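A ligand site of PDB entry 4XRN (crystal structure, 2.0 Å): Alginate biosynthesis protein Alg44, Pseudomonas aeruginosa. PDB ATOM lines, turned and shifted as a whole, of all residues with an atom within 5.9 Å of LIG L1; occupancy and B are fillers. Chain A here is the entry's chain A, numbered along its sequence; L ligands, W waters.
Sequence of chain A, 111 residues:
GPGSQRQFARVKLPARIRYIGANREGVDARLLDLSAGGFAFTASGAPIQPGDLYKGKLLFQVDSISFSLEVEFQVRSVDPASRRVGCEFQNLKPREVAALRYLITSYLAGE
The backbone carbonyl oxygen (O) of Asp 33 is in hydrogen-bond range of the backbone NH (N) of Ala 40 (3.2 Å).
OE1 of Glu 88 is in salt-bridge range of NE of Arg 76 (3.8 Å).
The backbone NH (N) of Arg 76 is in hydrogen-bond range of the backbone carbonyl oxygen (O) of Gly 86, 2.7 Å away.
The backbone NH (N) of Gly 37 lies close to the side-chain hydroxyl (OG) of Ser 35, at 3.1 Å.
The backbone carbonyl oxygen (O) of Gly 37 is in hydrogen-bond range of the backbone NH (N) of Phe 89 (3.0 Å).
O of Phe 39 is in hydrogen-bond range of N of Cys 87 (2.9 Å).
N of Gly 38 lies within hydrogen-bond range of OG of Ser 35 (3.2 Å).
N of Gly 86 is in hydrogen-bond range of O of Ser 77, 2.9 Å away.
Water W5 lies within hydrogen-bond range of O8 of LIG L1 (2.7 Å), OG of Ser 35 (2.7 Å), O of Phe 8 (2.8 Å) and NE of Arg 10 (3.2 Å).
Water W1 lies within hydrogen-bond range of the side-chain hydroxyl of Ser 77 (2.6 Å), a nitrogen (N2) of LIG L1 (2.8 Å) and a nitrogen (N3) of LG2 L2 (2.8 Å).
Water W3 bridges the side-chain carboxylate (OE2) of Glu 88 and an oxygen (O6) of LIG L1.
A nitrogen (N8) of LIG L1 is in hydrogen-bond range of an oxygen (O8) of LG2 L2 (2.8 Å).
The backbone NH (N) of Ser 35 sits close to a nitrogen (N4) of LIG L1 (3.4 Å).
N1 of LIG L1 sits close to O of Cys 87 (3.2 Å).
Residues that only touch LIG L1: Ser 4, Leu 34, Ala 40, Gly 86 and Glu 88.
Hydrophobic or aromatic side chains within 4 Å of LIG L1: Ala 40.
Within 4 Å of LIG L1: Ser 4, Arg 6, Gln 7, Arg 10, Asp 33, Leu 34, Ser 35, Gly 37, Gly 38, Phe 39, Ala 40, Arg 76, Arg 84, Gly 86, Cys 87 and Glu 88.
A nitrogen (N3) of LIG L1 is in hydrogen-bond range of the side-chain carboxylate (OD1) of Asp 33 (2.6 Å).
An oxygen (O9) of LIG L1 sits at hydrogen-bond distance from the backbone NH (N) of Gln 7 (2.6 Å).
An oxygen (O7) of LIG L1 sits at hydrogen-bond distance from the guanidinium group of Arg 84, 2.8 Å away.
NH2 of Arg 6 sits at hydrogen-bond distance from O14 of LIG L1 (2.9 Å).
O2 of LIG L1 lies within salt-bridge range of NE of Arg 76 (3.0 Å).
An oxygen (O6) of LIG L1 sits close to the backbone carbonyl oxygen (O) of Gly 37 (3.3 Å).
A nitrogen (N4) of LIG L1 sits at hydrogen-bond distance from the backbone carbonyl oxygen of Gly 38 (3.2 Å).
The guanidinium group of Arg 10 is in salt-bridge range of an oxygen (O8) of LIG L1 (3.2 Å).
N5 of LIG L1 lies within hydrogen-bond range of N of Phe 39, at 3.4 Å.
The guanidinium group (NH1) of Arg 84 lies within hydrogen-bond range of an oxygen (O4) of LG2 L2 (3.1 Å).
The guanidinium group (NH2) of Arg 6 is in salt-bridge range of an oxygen (O1) of LG2 L2, at 2.9 Å.
N2 of LG2 L2 lies within hydrogen-bond range of NH1 of Arg 10 (2.9 Å).
The backbone NH of Ser 4 sits at hydrogen-bond distance from an oxygen (O14) of LG2 L2 (3.0 Å).
A nitrogen (N8) of LG2 L2 lies within hydrogen-bond range of the backbone carbonyl oxygen (O) of Ser 4 (2.8 Å).
A nitrogen (N5) of LG2 L2 sits at hydrogen-bond distance from the side-chain hydroxyl (OG) of Ser 77 (3.4 Å).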
ATOM      1  N   SER A   4     -25.535   6.316 -31.402  1.00  0.00           N
ATOM      2  CA  SER A   4     -25.534   6.502 -29.951  1.00  0.00           C
ATOM      3  C   SER A   4     -24.245   5.983 -29.353  1.00  0.00           C
ATOM      4  O   SER A   4     -23.649   5.029 -29.855  1.00  0.00           O
ATOM      5  CB  SER A   4     -26.713   5.783 -29.291  1.00  0.00           C
ATOM      6  OG  SER A   4     -27.928   5.984 -30.009  1.00  0.00           O
ATOM      7  N   GLN A   5     -23.806   6.619 -28.273  1.00  0.00           N
ATOM      8  CA  GLN A   5     -22.636   6.087 -27.618  1.00  0.00           C
ATOM      9  C   GLN A   5     -23.124   5.004 -26.651  1.00  0.00           C
ATOM     10  O   GLN A   5     -23.990   5.251 -25.809  1.00  0.00           O
ATOM     11  CB  GLN A   5     -21.811   7.162 -26.906  1.00  0.00           C
ATOM     12  CG  GLN A   5     -20.347   6.742 -26.791  1.00  0.00           C
ATOM     13  CD  GLN A   5     -19.433   7.760 -26.165  1.00  0.00           C
ATOM     14  OE1 GLN A   5     -19.649   8.966 -26.268  1.00  0.00           O
ATOM     15  NE2 GLN A   5     -18.408   7.289 -25.470  1.00  0.00           N
ATOM     16  N   ARG A   6     -22.593   3.803 -26.808  1.00  0.00           N
ATOM     17  CA  ARG A   6     -22.985   2.702 -25.961  1.00  0.00           C
ATOM     18  C   ARG A   6     -22.428   2.954 -24.579  1.00  0.00           C
ATOM     19  O   ARG A   6     -21.239   3.274 -24.435  1.00  0.00           O
ATOM     20  CB  ARG A   6     -22.483   1.378 -26.516  1.00  0.00           C
ATOM     21  CG  ARG A   6     -23.051   1.069 -27.891  1.00  0.00           C
ATOM     22  CD  ARG A   6     -22.118   0.175 -28.669  1.00  0.00           C
ATOM     23  NE  ARG A   6     -22.714  -0.336 -29.891  1.00  0.00           N
ATOM     24  CZ  ARG A   6     -22.165  -1.273 -30.646  1.00  0.00           C
ATOM     25  NH1 ARG A   6     -20.987  -1.784 -30.288  1.00  0.00           N
ATOM     26  NH2 ARG A   6     -22.774  -1.709 -31.738  1.00  0.00           N
ATOM     27  N   GLN A   7     -23.273   2.845 -23.571  1.00  0.00           N
ATOM     28  CA  GLN A   7     -22.836   3.103 -22.203  1.00  0.00           C
ATOM     29  C   GLN A   7     -21.753   2.120 -21.753  1.00  0.00           C
ATOM     30  O   GLN A   7     -20.879   2.470 -20.963  1.00  0.00           O
ATOM     31  CB  GLN A   7     -24.037   3.047 -21.263  1.00  0.00           C
ATOM     32  CG  GLN A   7     -23.705   3.349 -19.830  1.00  0.00           C
ATOM     33  CD  GLN A   7     -24.917   3.243 -18.947  1.00  0.00           C
ATOM     34  OE1 GLN A   7     -26.052   3.259 -19.433  1.00  0.00           O
ATOM     35  NE2 GLN A   7     -24.693   3.154 -17.645  1.00  0.00           N
ATOM     36  N   PHE A   8     -21.793   0.892 -22.278  1.00  0.00           N
ATOM     37  CA  PHE A   8     -20.818  -0.138 -21.914  1.00  0.00           C
ATOM     38  C   PHE A   8     -20.166  -0.703 -23.161  1.00  0.00           C
ATOM     39  O   PHE A   8     -20.807  -0.843 -24.194  1.00  0.00           O
ATOM     40  CB  PHE A   8     -21.507  -1.270 -21.119  1.00  0.00           C
ATOM     41  CG  PHE A   8     -22.308  -0.781 -19.963  1.00  0.00           C
ATOM     42  CD1 PHE A   8     -21.694  -0.482 -18.748  1.00  0.00           C
ATOM     43  CD2 PHE A   8     -23.669  -0.586 -20.083  1.00  0.00           C
ATOM     44  CE1 PHE A   8     -22.440   0.000 -17.673  1.00  0.00           C
ATOM     45  CE2 PHE A   8     -24.415  -0.103 -19.009  1.00  0.00           C
ATOM     46  CZ  PHE A   8     -23.810   0.174 -17.815  1.00  0.00           C
ATOM     47  N   ARG A  10     -18.533  -3.368 -25.738  1.00  0.00           N
ATOM     48  CA  ARG A  10     -18.909  -4.730 -26.111  1.00  0.00           C
ATOM     49  C   ARG A  10     -17.722  -5.496 -26.654  1.00  0.00           C
ATOM     50  O   ARG A  10     -16.874  -4.920 -27.331  1.00  0.00           O
ATOM     51  CB  ARG A  10     -20.029  -4.690 -27.150  1.00  0.00           C
ATOM     52  CG  ARG A  10     -21.139  -3.751 -26.821  1.00  0.00           C
ATOM     53  CD  ARG A  10     -22.271  -3.901 -27.815  1.00  0.00           C
ATOM     54  NE  ARG A  10     -23.398  -3.054 -27.479  1.00  0.00           N
ATOM     55  CZ  ARG A  10     -24.489  -2.923 -28.228  1.00  0.00           C
ATOM     56  NH1 ARG A  10     -24.577  -3.591 -29.367  1.00  0.00           N
ATOM     57  NH2 ARG A  10     -25.475  -2.120 -27.839  1.00  0.00           N
ATOM     58  N   VAL A  11     -17.648  -6.784 -26.351  1.00  0.00           N
ATOM     59  CA  VAL A  11     -16.545  -7.603 -26.805  1.00  0.00           C
ATOM     60  C   VAL A  11     -17.028  -8.966 -27.284  1.00  0.00           C
ATOM     61  O   VAL A  11     -18.081  -9.444 -26.853  1.00  0.00           O
ATOM     62  CB  VAL A  11     -15.491  -7.834 -25.709  1.00  0.00           C
ATOM     63  CG1 VAL A  11     -14.955  -6.491 -25.185  1.00  0.00           C
ATOM     64  CG2 VAL A  11     -16.065  -8.673 -24.574  1.00  0.00           C
ATOM     65  N   ASP A  33     -21.902 -11.010 -28.937  1.00  0.00           N
ATOM     66  CA  ASP A  33     -21.030 -10.170 -28.121  1.00  0.00           C
ATOM     67  C   ASP A  33     -21.624 -10.007 -26.746  1.00  0.00           C
ATOM     68  O   ASP A  33     -22.754 -10.447 -26.486  1.00  0.00           O
ATOM     69  CB  ASP A  33     -20.788  -8.795 -28.760  1.00  0.00           C
ATOM     70  CG  ASP A  33     -22.073  -8.086 -29.176  1.00  0.00           C
ATOM     71  OD1 ASP A  33     -22.874  -7.715 -28.300  1.00  0.00           O
ATOM     72  OD2 ASP A  33     -22.254  -7.870 -30.400  1.00  0.00           O
ATOM     73  N   LEU A  34     -20.866  -9.350 -25.885  1.00  0.00           N
ATOM     74  CA  LEU A  34     -21.240  -9.160 -24.495  1.00  0.00           C
ATOM     75  C   LEU A  34     -20.723  -7.839 -23.955  1.00  0.00           C
ATOM     76  O   LEU A  34     -19.601  -7.432 -24.258  1.00  0.00           O
ATOM     77  CB  LEU A  34     -20.714 -10.314 -23.651  1.00  0.00           C
ATOM     78  CG  LEU A  34     -20.849 -10.190 -22.137  1.00  0.00           C
ATOM     79  CD1 LEU A  34     -22.314 -10.374 -21.700  1.00  0.00           C
ATOM     80  CD2 LEU A  34     -19.958 -11.207 -21.455  1.00  0.00           C
ATOM     81  N   SER A  35     -21.546  -7.165 -23.162  1.00  0.00           N
ATOM     82  CA  SER A  35     -21.110  -5.993 -22.408  1.00  0.00           C
ATOM     83  C   SER A  35     -21.683  -6.101 -20.999  1.00  0.00           C
ATOM     84  O   SER A  35     -22.403  -7.046 -20.693  1.00  0.00           O
ATOM     85  CB  SER A  35     -21.566  -4.696 -23.061  1.00  0.00           C
ATOM     86  OG  SER A  35     -22.971  -4.539 -22.959  1.00  0.00           O
ATOM     87  N   ALA A  36     -21.407  -5.105 -20.155  1.00  0.00           N
ATOM     88  CA  ALA A  36     -21.947  -5.101 -18.808  1.00  0.00           C
ATOM     89  C   ALA A  36     -23.419  -4.728 -18.824  1.00  0.00           C
ATOM     90  O   ALA A  36     -24.117  -4.870 -17.833  1.00  0.00           O
ATOM     91  CB  ALA A  36     -21.162  -4.157 -17.913  1.00  0.00           C
ATOM     92  N   GLY A  37     -23.883  -4.250 -19.973  1.00  0.00           N
ATOM     93  CA  GLY A  37     -25.257  -3.848 -20.115  1.00  0.00           C
ATOM     94  C   GLY A  37     -26.129  -4.906 -20.774  1.00  0.00           C
ATOM     95  O   GLY A  37     -27.361  -4.874 -20.658  1.00  0.00           O
ATOM     96  N   GLY A  38     -25.504  -5.856 -21.477  1.00  0.00           N
ATOM     97  CA  GLY A  38     -26.256  -6.836 -22.226  1.00  0.00           C
ATOM     98  C   GLY A  38     -25.464  -7.671 -23.213  1.00  0.00           C
ATOM     99  O   GLY A  38     -24.241  -7.776 -23.124  1.00  0.00           O
ATOM    100  N   PHE A  39     -26.167  -8.276 -24.169  1.00  0.00           N
ATOM    101  CA  PHE A  39     -25.557  -9.238 -25.055  1.00  0.00           C
ATOM    102  C   PHE A  39     -26.373  -9.424 -26.326  1.00  0.00           C
ATOM    103  O   PHE A  39     -27.507  -8.977 -26.440  1.00  0.00           O
ATOM    104  CB  PHE A  39     -25.391 -10.599 -24.336  1.00  0.00           C
ATOM    105  CG  PHE A  39     -26.692 -11.221 -23.899  1.00  0.00           C
ATOM    106  CD1 PHE A  39     -27.266 -10.877 -22.684  1.00  0.00           C
ATOM    107  CD2 PHE A  39     -27.337 -12.158 -24.704  1.00  0.00           C
ATOM    108  CE1 PHE A  39     -28.495 -11.451 -22.265  1.00  0.00           C
ATOM    109  CE2 PHE A  39     -28.543 -12.735 -24.301  1.00  0.00           C
ATOM    110  CZ  PHE A  39     -29.119 -12.379 -23.078  1.00  0.00           C
ATOM    111  N   ALA A  40     -25.791 -10.118 -27.281  1.00  0.00           N
ATOM    112  CA  ALA A  40     -26.524 -10.441 -28.490  1.00  0.00           C
ATOM    113  C   ALA A  40     -26.282 -11.882 -28.848  1.00  0.00           C
ATOM    114  O   ALA A  40     -25.234 -12.426 -28.511  1.00  0.00           O
ATOM    115  CB  ALA A  40     -26.102  -9.526 -29.649  1.00  0.00           C
ATOM    116  N   ARG A  76     -34.368  -6.284 -26.616  1.00  0.00           N
ATOM    117  CA  ARG A  76     -34.471  -4.885 -27.048  1.00  0.00           C
ATOM    118  C   ARG A  76     -34.699  -4.780 -28.547  1.00  0.00           C
ATOM    119  O   ARG A  76     -35.370  -3.857 -29.012  1.00  0.00           O
ATOM    120  CB  ARG A  76     -33.205  -4.084 -26.669  1.00  0.00           C
ATOM    121  CG  ARG A  76     -32.952  -3.988 -25.173  1.00  0.00           C
ATOM    122  CD  ARG A  76     -34.147  -3.394 -24.429  1.00  0.00           C
ATOM    123  NE  ARG A  76     -34.431  -2.038 -24.879  1.00  0.00           N
ATOM    124  CZ  ARG A  76     -35.379  -1.266 -24.351  1.00  0.00           C
ATOM    125  NH1 ARG A  76     -36.121  -1.717 -23.351  1.00  0.00           N
ATOM    126  NH2 ARG A  76     -35.573  -0.045 -24.817  1.00  0.00           N
ATOM    127  N   SER A  77     -34.143  -5.724 -29.302  1.00  0.00           N
ATOM    128  CA  SER A  77     -34.310  -5.705 -30.758  1.00  0.00           C
ATOM    129  C   SER A  77     -34.180  -7.097 -31.355  1.00  0.00           C
ATOM    130  O   SER A  77     -33.461  -7.946 -30.821  1.00  0.00           O
ATOM    131  CB  SER A  77     -33.283  -4.771 -31.395  1.00  0.00           C
ATOM    132  OG  SER A  77     -31.956  -5.225 -31.209  1.00  0.00           O
ATOM    133  N   ARG A  84     -30.861 -11.776 -35.419  1.00  0.00           N
ATOM    134  CA  ARG A  84     -29.990 -11.220 -34.383  1.00  0.00           C
ATOM    135  C   ARG A  84     -30.839 -10.676 -33.258  1.00  0.00           C
ATOM    136  O   ARG A  84     -31.699  -9.829 -33.478  1.00  0.00           O
ATOM    137  CB  ARG A  84     -29.098 -10.116 -34.922  1.00  0.00           C
ATOM    138  CG  ARG A  84     -28.019  -9.700 -33.932  1.00  0.00           C
ATOM    139  CD  ARG A  84     -27.188  -8.558 -34.480  1.00  0.00           C
ATOM    140  NE  ARG A  84     -26.107  -8.206 -33.563  1.00  0.00           N
ATOM    141  CZ  ARG A  84     -26.273  -7.464 -32.484  1.00  0.00           C
ATOM    142  NH1 ARG A  84     -27.481  -6.990 -32.167  1.00  0.00           N
ATOM    143  NH2 ARG A  84     -25.221  -7.188 -31.708  1.00  0.00           N
ATOM    144  N   VAL A  85     -30.607 -11.156 -32.045  1.00  0.00           N
ATOM    145  CA  VAL A  85     -31.353 -10.681 -30.893  1.00  0.00           C
ATOM    146  C   VAL A  85     -30.441  -9.849 -30.016  1.00  0.00           C
ATOM    147  O   VAL A  85     -29.376 -10.308 -29.621  1.00  0.00           O
ATOM    148  CB  VAL A  85     -31.939 -11.852 -30.078  1.00  0.00           C
ATOM    149  CG1 VAL A  85     -32.890 -11.340 -28.997  1.00  0.00           C
ATOM    150  CG2 VAL A  85     -32.655 -12.823 -30.992  1.00  0.00           C
ATOM    151  N   GLY A  86     -30.853  -8.608 -29.730  1.00  0.00           N
ATOM    152  CA  GLY A  86     -30.111  -7.769 -28.814  1.00  0.00           C
ATOM    153  C   GLY A  86     -30.860  -7.675 -27.516  1.00  0.00           C
ATOM    154  O   GLY A  86     -32.058  -7.406 -27.524  1.00  0.00           O
ATOM    155  N   CYS A  87     -30.161  -7.889 -26.389  1.00  0.00           N
ATOM    156  CA  CYS A  87     -30.794  -8.023 -25.076  1.00  0.00           C
ATOM    157  C   CYS A  87     -30.169  -7.116 -24.016  1.00  0.00           C
ATOM    158  O   CYS A  87     -28.980  -6.775 -24.105  1.00  0.00           O
ATOM    159  CB  CYS A  87     -30.720  -9.471 -24.601  1.00  0.00           C
ATOM    160  SG  CYS A  87     -31.479 -10.661 -25.689  1.00  0.00           S
ATOM    161  N   GLU A  88     -30.963  -6.736 -23.019  1.00  0.00           N
ATOM    162  CA  GLU A  88     -30.466  -5.864 -21.951  1.00  0.00           C
ATOM    163  C   GLU A  88     -30.688  -6.513 -20.600  1.00  0.00           C
ATOM    164  O   GLU A  88     -31.809  -6.920 -20.297  1.00  0.00           O
ATOM    165  CB  GLU A  88     -31.161  -4.513 -21.978  1.00  0.00           C
ATOM    166  CG  GLU A  88     -30.687  -3.549 -20.899  1.00  0.00           C
ATOM    167  CD  GLU A  88     -31.369  -2.194 -20.983  1.00  0.00           C
ATOM    168  OE1 GLU A  88     -32.441  -2.096 -21.634  1.00  0.00           O
ATOM    169  OE2 GLU A  88     -30.815  -1.227 -20.434  1.00  0.00           O
ATOM    170  N   PHE A  89     -29.621  -6.600 -19.806  1.00  0.00           N
ATOM    171  CA  PHE A  89     -29.689  -7.132 -18.455  1.00  0.00           C
ATOM    172  C   PHE A  89     -30.628  -6.279 -17.614  1.00  0.00           C
ATOM    173  O   PHE A  89     -30.607  -5.055 -17.725  1.00  0.00           O
ATOM    174  CB  PHE A  89     -28.295  -7.154 -17.801  1.00  0.00           C
ATOM    175  CG  PHE A  89     -27.334  -8.118 -18.447  1.00  0.00           C
ATOM    176  CD1 PHE A  89     -27.720  -9.410 -18.761  1.00  0.00           C
ATOM    177  CD2 PHE A  89     -26.031  -7.726 -18.734  1.00  0.00           C
ATOM    178  CE1 PHE A  89     -26.835 -10.301 -19.344  1.00  0.00           C
ATOM    179  CE2 PHE A  89     -25.139  -8.594 -19.324  1.00  0.00           C
ATOM    180  CZ  PHE A  89     -25.533  -9.879 -19.637  1.00  0.00           C
HETATM  181  P1  LIG L   1     -31.144  -0.464 -27.013  1.00  0.00           P
HETATM  182  O1  LIG L   1     -31.309  -1.106 -28.373  1.00  0.00           O
HETATM  183  O2  LIG L   1     -32.515  -0.350 -26.383  1.00  0.00           O
HETATM  184  O3  LIG L   1     -30.252  -1.418 -25.911  1.00  0.00           O
HETATM  185  C1  LIG L   1     -30.262  -0.961 -24.531  1.00  0.00           C
HETATM  186  C2  LIG L   1     -28.953  -1.613 -23.838  1.00  0.00           C
HETATM  187  O4  LIG L   1     -29.163  -3.162 -23.928  1.00  0.00           O
HETATM  188  C3  LIG L   1     -27.958  -1.380 -24.484  1.00  0.00           C
HETATM  189  O5  LIG L   1     -27.228  -0.160 -23.890  1.00  0.00           O
HETATM  190  C4  LIG L   1     -27.025  -2.724 -24.182  1.00  0.00           C
HETATM  191  O6  LIG L   1     -26.474  -2.575 -22.853  1.00  0.00           O
HETATM  192  C5  LIG L   1     -27.810  -3.717 -24.243  1.00  0.00           C
HETATM  193  N1  LIG L   1     -27.947  -4.222 -25.665  1.00  0.00           N
HETATM  194  C6  LIG L   1     -28.932  -4.109 -26.583  1.00  0.00           C
HETATM  195  N2  LIG L   1     -28.524  -4.740 -27.696  1.00  0.00           N
HETATM  196  C7  LIG L   1     -27.303  -5.237 -27.469  1.00  0.00           C
HETATM  197  C8  LIG L   1     -26.336  -6.030 -28.331  1.00  0.00           C
HETATM  198  O7  LIG L   1     -26.631  -6.324 -29.433  1.00  0.00           O
HETATM  199  N3  LIG L   1     -25.070  -6.422 -27.792  1.00  0.00           N
HETATM  200  C9  LIG L   1     -24.722  -6.051 -26.451  1.00  0.00           C
HETATM  201  N4  LIG L   1     -23.460  -6.449 -25.891  1.00  0.00           N
HETATM  202  N5  LIG L   1     -25.656  -5.292 -25.634  1.00  0.00           N
HETATM  203  C10 LIG L   1     -26.944  -4.890 -26.207  1.00  0.00           C
HETATM  204  P2  LIG L   1     -26.042   0.530 -24.941  1.00  0.00           P
HETATM  205  O8  LIG L   1     -24.807  -0.275 -25.304  1.00  0.00           O
HETATM  206  O9  LIG L   1     -25.552   1.759 -24.197  1.00  0.00           O
HETATM  207  O10 LIG L   1     -26.967   1.031 -26.230  1.00  0.00           O
HETATM  208  C11 LIG L   1     -27.805   2.129 -25.949  1.00  0.00           C
HETATM  209  C12 LIG L   1     -28.502   2.477 -27.086  1.00  0.00           C
HETATM  210  O11 LIG L   1     -27.580   2.799 -28.249  1.00  0.00           O
HETATM  211  C13 LIG L   1     -29.328   1.231 -27.688  1.00  0.00           C
HETATM  212  O12 LIG L   1     -30.671   1.135 -26.988  1.00  0.00           O
HETATM  213  C14 LIG L   1     -29.502   1.480 -28.897  1.00  0.00           C
HETATM  214  O13 LIG L   1     -30.730   2.276 -29.130  1.00  0.00           O
HETATM  215  C15 LIG L   1     -28.174   2.379 -29.335  1.00  0.00           C
HETATM  216  N6  LIG L   1     -27.298   1.598 -30.120  1.00  0.00           N
HETATM  217  C16 LIG L   1     -26.082   1.301 -29.597  1.00  0.00           C
HETATM  218  N7  LIG L   1     -25.411   0.582 -30.530  1.00  0.00           N
HETATM  219  C17 LIG L   1     -26.203   0.448 -31.624  1.00  0.00           C
HETATM  220  C18 LIG L   1     -26.022  -0.251 -32.993  1.00  0.00           C
HETATM  221  O14 LIG L   1     -25.009  -0.803 -33.278  1.00  0.00           O
HETATM  222  N8  LIG L   1     -27.084  -0.231 -33.945  1.00  0.00           N
HETATM  223  C19 LIG L   1     -28.324   0.458 -33.642  1.00  0.00           C
HETATM  224  N9  LIG L   1     -29.427   0.496 -34.619  1.00  0.00           N
HETATM  225  N10 LIG L   1     -28.485   1.114 -32.360  1.00  0.00           N
HETATM  226  C20 LIG L   1     -27.374   1.081 -31.348  1.00  0.00           C
HETATM  227  P1  LG2 L   2     -22.442  -4.648 -34.798  1.00  0.00           P
HETATM  228  O1  LG2 L   2     -22.352  -3.984 -33.440  1.00  0.00           O
HETATM  229  O2  LG2 L   2     -21.566  -5.879 -34.808  1.00  0.00           O
HETATM  230  O3  LG2 L   2     -23.901  -5.279 -35.280  1.00  0.00           O
HETATM  231  C1  LG2 L   2     -24.913  -4.355 -34.915  1.00  0.00           C
HETATM  232  C2  LG2 L   2     -26.240  -4.608 -35.772  1.00  0.00           C
HETATM  233  O4  LG2 L   2     -27.254  -5.328 -34.803  1.00  0.00           O
HETATM  234  C3  LG2 L   2     -26.636  -3.468 -35.950  1.00  0.00           C
HETATM  235  O5  LG2 L   2     -26.510  -3.036 -37.436  1.00  0.00           O
HETATM  236  C4  LG2 L   2     -28.183  -3.392 -35.331  1.00  0.00           C
HETATM  237  O6  LG2 L   2     -29.162  -3.728 -36.354  1.00  0.00           O
HETATM  238  C5  LG2 L   2     -28.218  -4.242 -34.401  1.00  0.00           C
HETATM  239  N1  LG2 L   2     -27.727  -3.647 -33.071  1.00  0.00           N
HETATM  240  C6  LG2 L   2     -26.519  -3.612 -32.460  1.00  0.00           C
HETATM  241  N2  LG2 L   2     -26.642  -2.948 -31.315  1.00  0.00           N
HETATM  242  C7  LG2 L   2     -27.905  -2.584 -31.210  1.00  0.00           C
HETATM  243  C8  LG2 L   2     -28.649  -1.810 -30.129  1.00  0.00           C
HETATM  244  O7  LG2 L   2     -28.052  -1.446 -29.180  1.00  0.00           O
HETATM  245  N3  LG2 L   2     -30.042  -1.557 -30.295  1.00  0.00           N
HETATM  246  C9  LG2 L   2     -30.720  -2.028 -31.468  1.00  0.00           C
HETATM  247  N4  LG2 L   2     -32.123  -1.796 -31.684  1.00  0.00           N
HETATM  248  N5  LG2 L   2     -30.003  -2.764 -32.483  1.00  0.00           N
HETATM  249  C10 LG2 L   2     -28.568  -3.018 -32.306  1.00  0.00           C
HETATM  250  P2  LG2 L   2     -26.294  -1.321 -37.497  1.00  0.00           P
HETATM  251  O8  LG2 L   2     -27.253  -0.471 -36.698  1.00  0.00           O
HETATM  252  O9  LG2 L   2     -26.467  -0.945 -38.958  1.00  0.00           O
HETATM  253  O10 LG2 L   2     -24.690  -1.190 -37.059  1.00  0.00           O
HETATM  254  C11 LG2 L   2     -23.782  -1.780 -37.948  1.00  0.00           C
HETATM  255  C12 LG2 L   2     -22.527  -1.675 -37.409  1.00  0.00           C
HETATM  256  O11 LG2 L   2     -22.115  -0.227 -37.242  1.00  0.00           O
HETATM  257  C13 LG2 L   2     -22.438  -2.273 -35.913  1.00  0.00           C
HETATM  258  O12 LG2 L   2     -21.766  -3.654 -35.978  1.00  0.00           O
HETATM  259  C14 LG2 L   2     -21.711  -1.515 -35.232  1.00  0.00           C
HETATM  260  O13 LG2 L   2     -20.294  -1.915 -35.255  1.00  0.00           O
HETATM  261  C15 LG2 L   2     -21.735  -0.046 -35.993  1.00  0.00           C
HETATM  262  N6  LG2 L   2     -22.586   0.825 -35.278  1.00  0.00           N
HETATM  263  C16 LG2 L   2     -23.735   1.172 -35.889  1.00  0.00           C
HETATM  264  N7  LG2 L   2     -24.358   2.008 -35.048  1.00  0.00           N
HETATM  265  C17 LG2 L   2     -23.641   2.195 -33.962  1.00  0.00           C
HETATM  266  C18 LG2 L   2     -23.880   3.032 -32.706  1.00  0.00           C
HETATM  267  O14 LG2 L   2     -24.882   3.673 -32.625  1.00  0.00           O
HETATM  268  N8  LG2 L   2     -22.909   3.025 -31.663  1.00  0.00           N
HETATM  269  C19 LG2 L   2     -21.714   2.216 -31.818  1.00  0.00           C
HETATM  270  N9  LG2 L   2     -20.682   2.171 -30.780  1.00  0.00           N
HETATM  271  N10 LG2 L   2     -21.510   1.424 -33.021  1.00  0.00           N
HETATM  272  C20 LG2 L   2     -22.520   1.438 -34.097  1.00  0.00           C
HETATM  273  O   HOH W   1     -30.798  -4.079 -29.220  1.00  0.00           O
HETATM  274  O   HOH W   2     -33.810  -0.476 -28.854  1.00  0.00           O
HETATM  275  O   HOH W   3     -28.334  -1.125 -20.711  1.00  0.00           O
HETATM  276  O   HOH W   4     -32.169   1.373 -33.768  1.00  0.00           O
HETATM  277  O   HOH W   5     -23.243  -2.263 -24.400  1.00  0.00           O
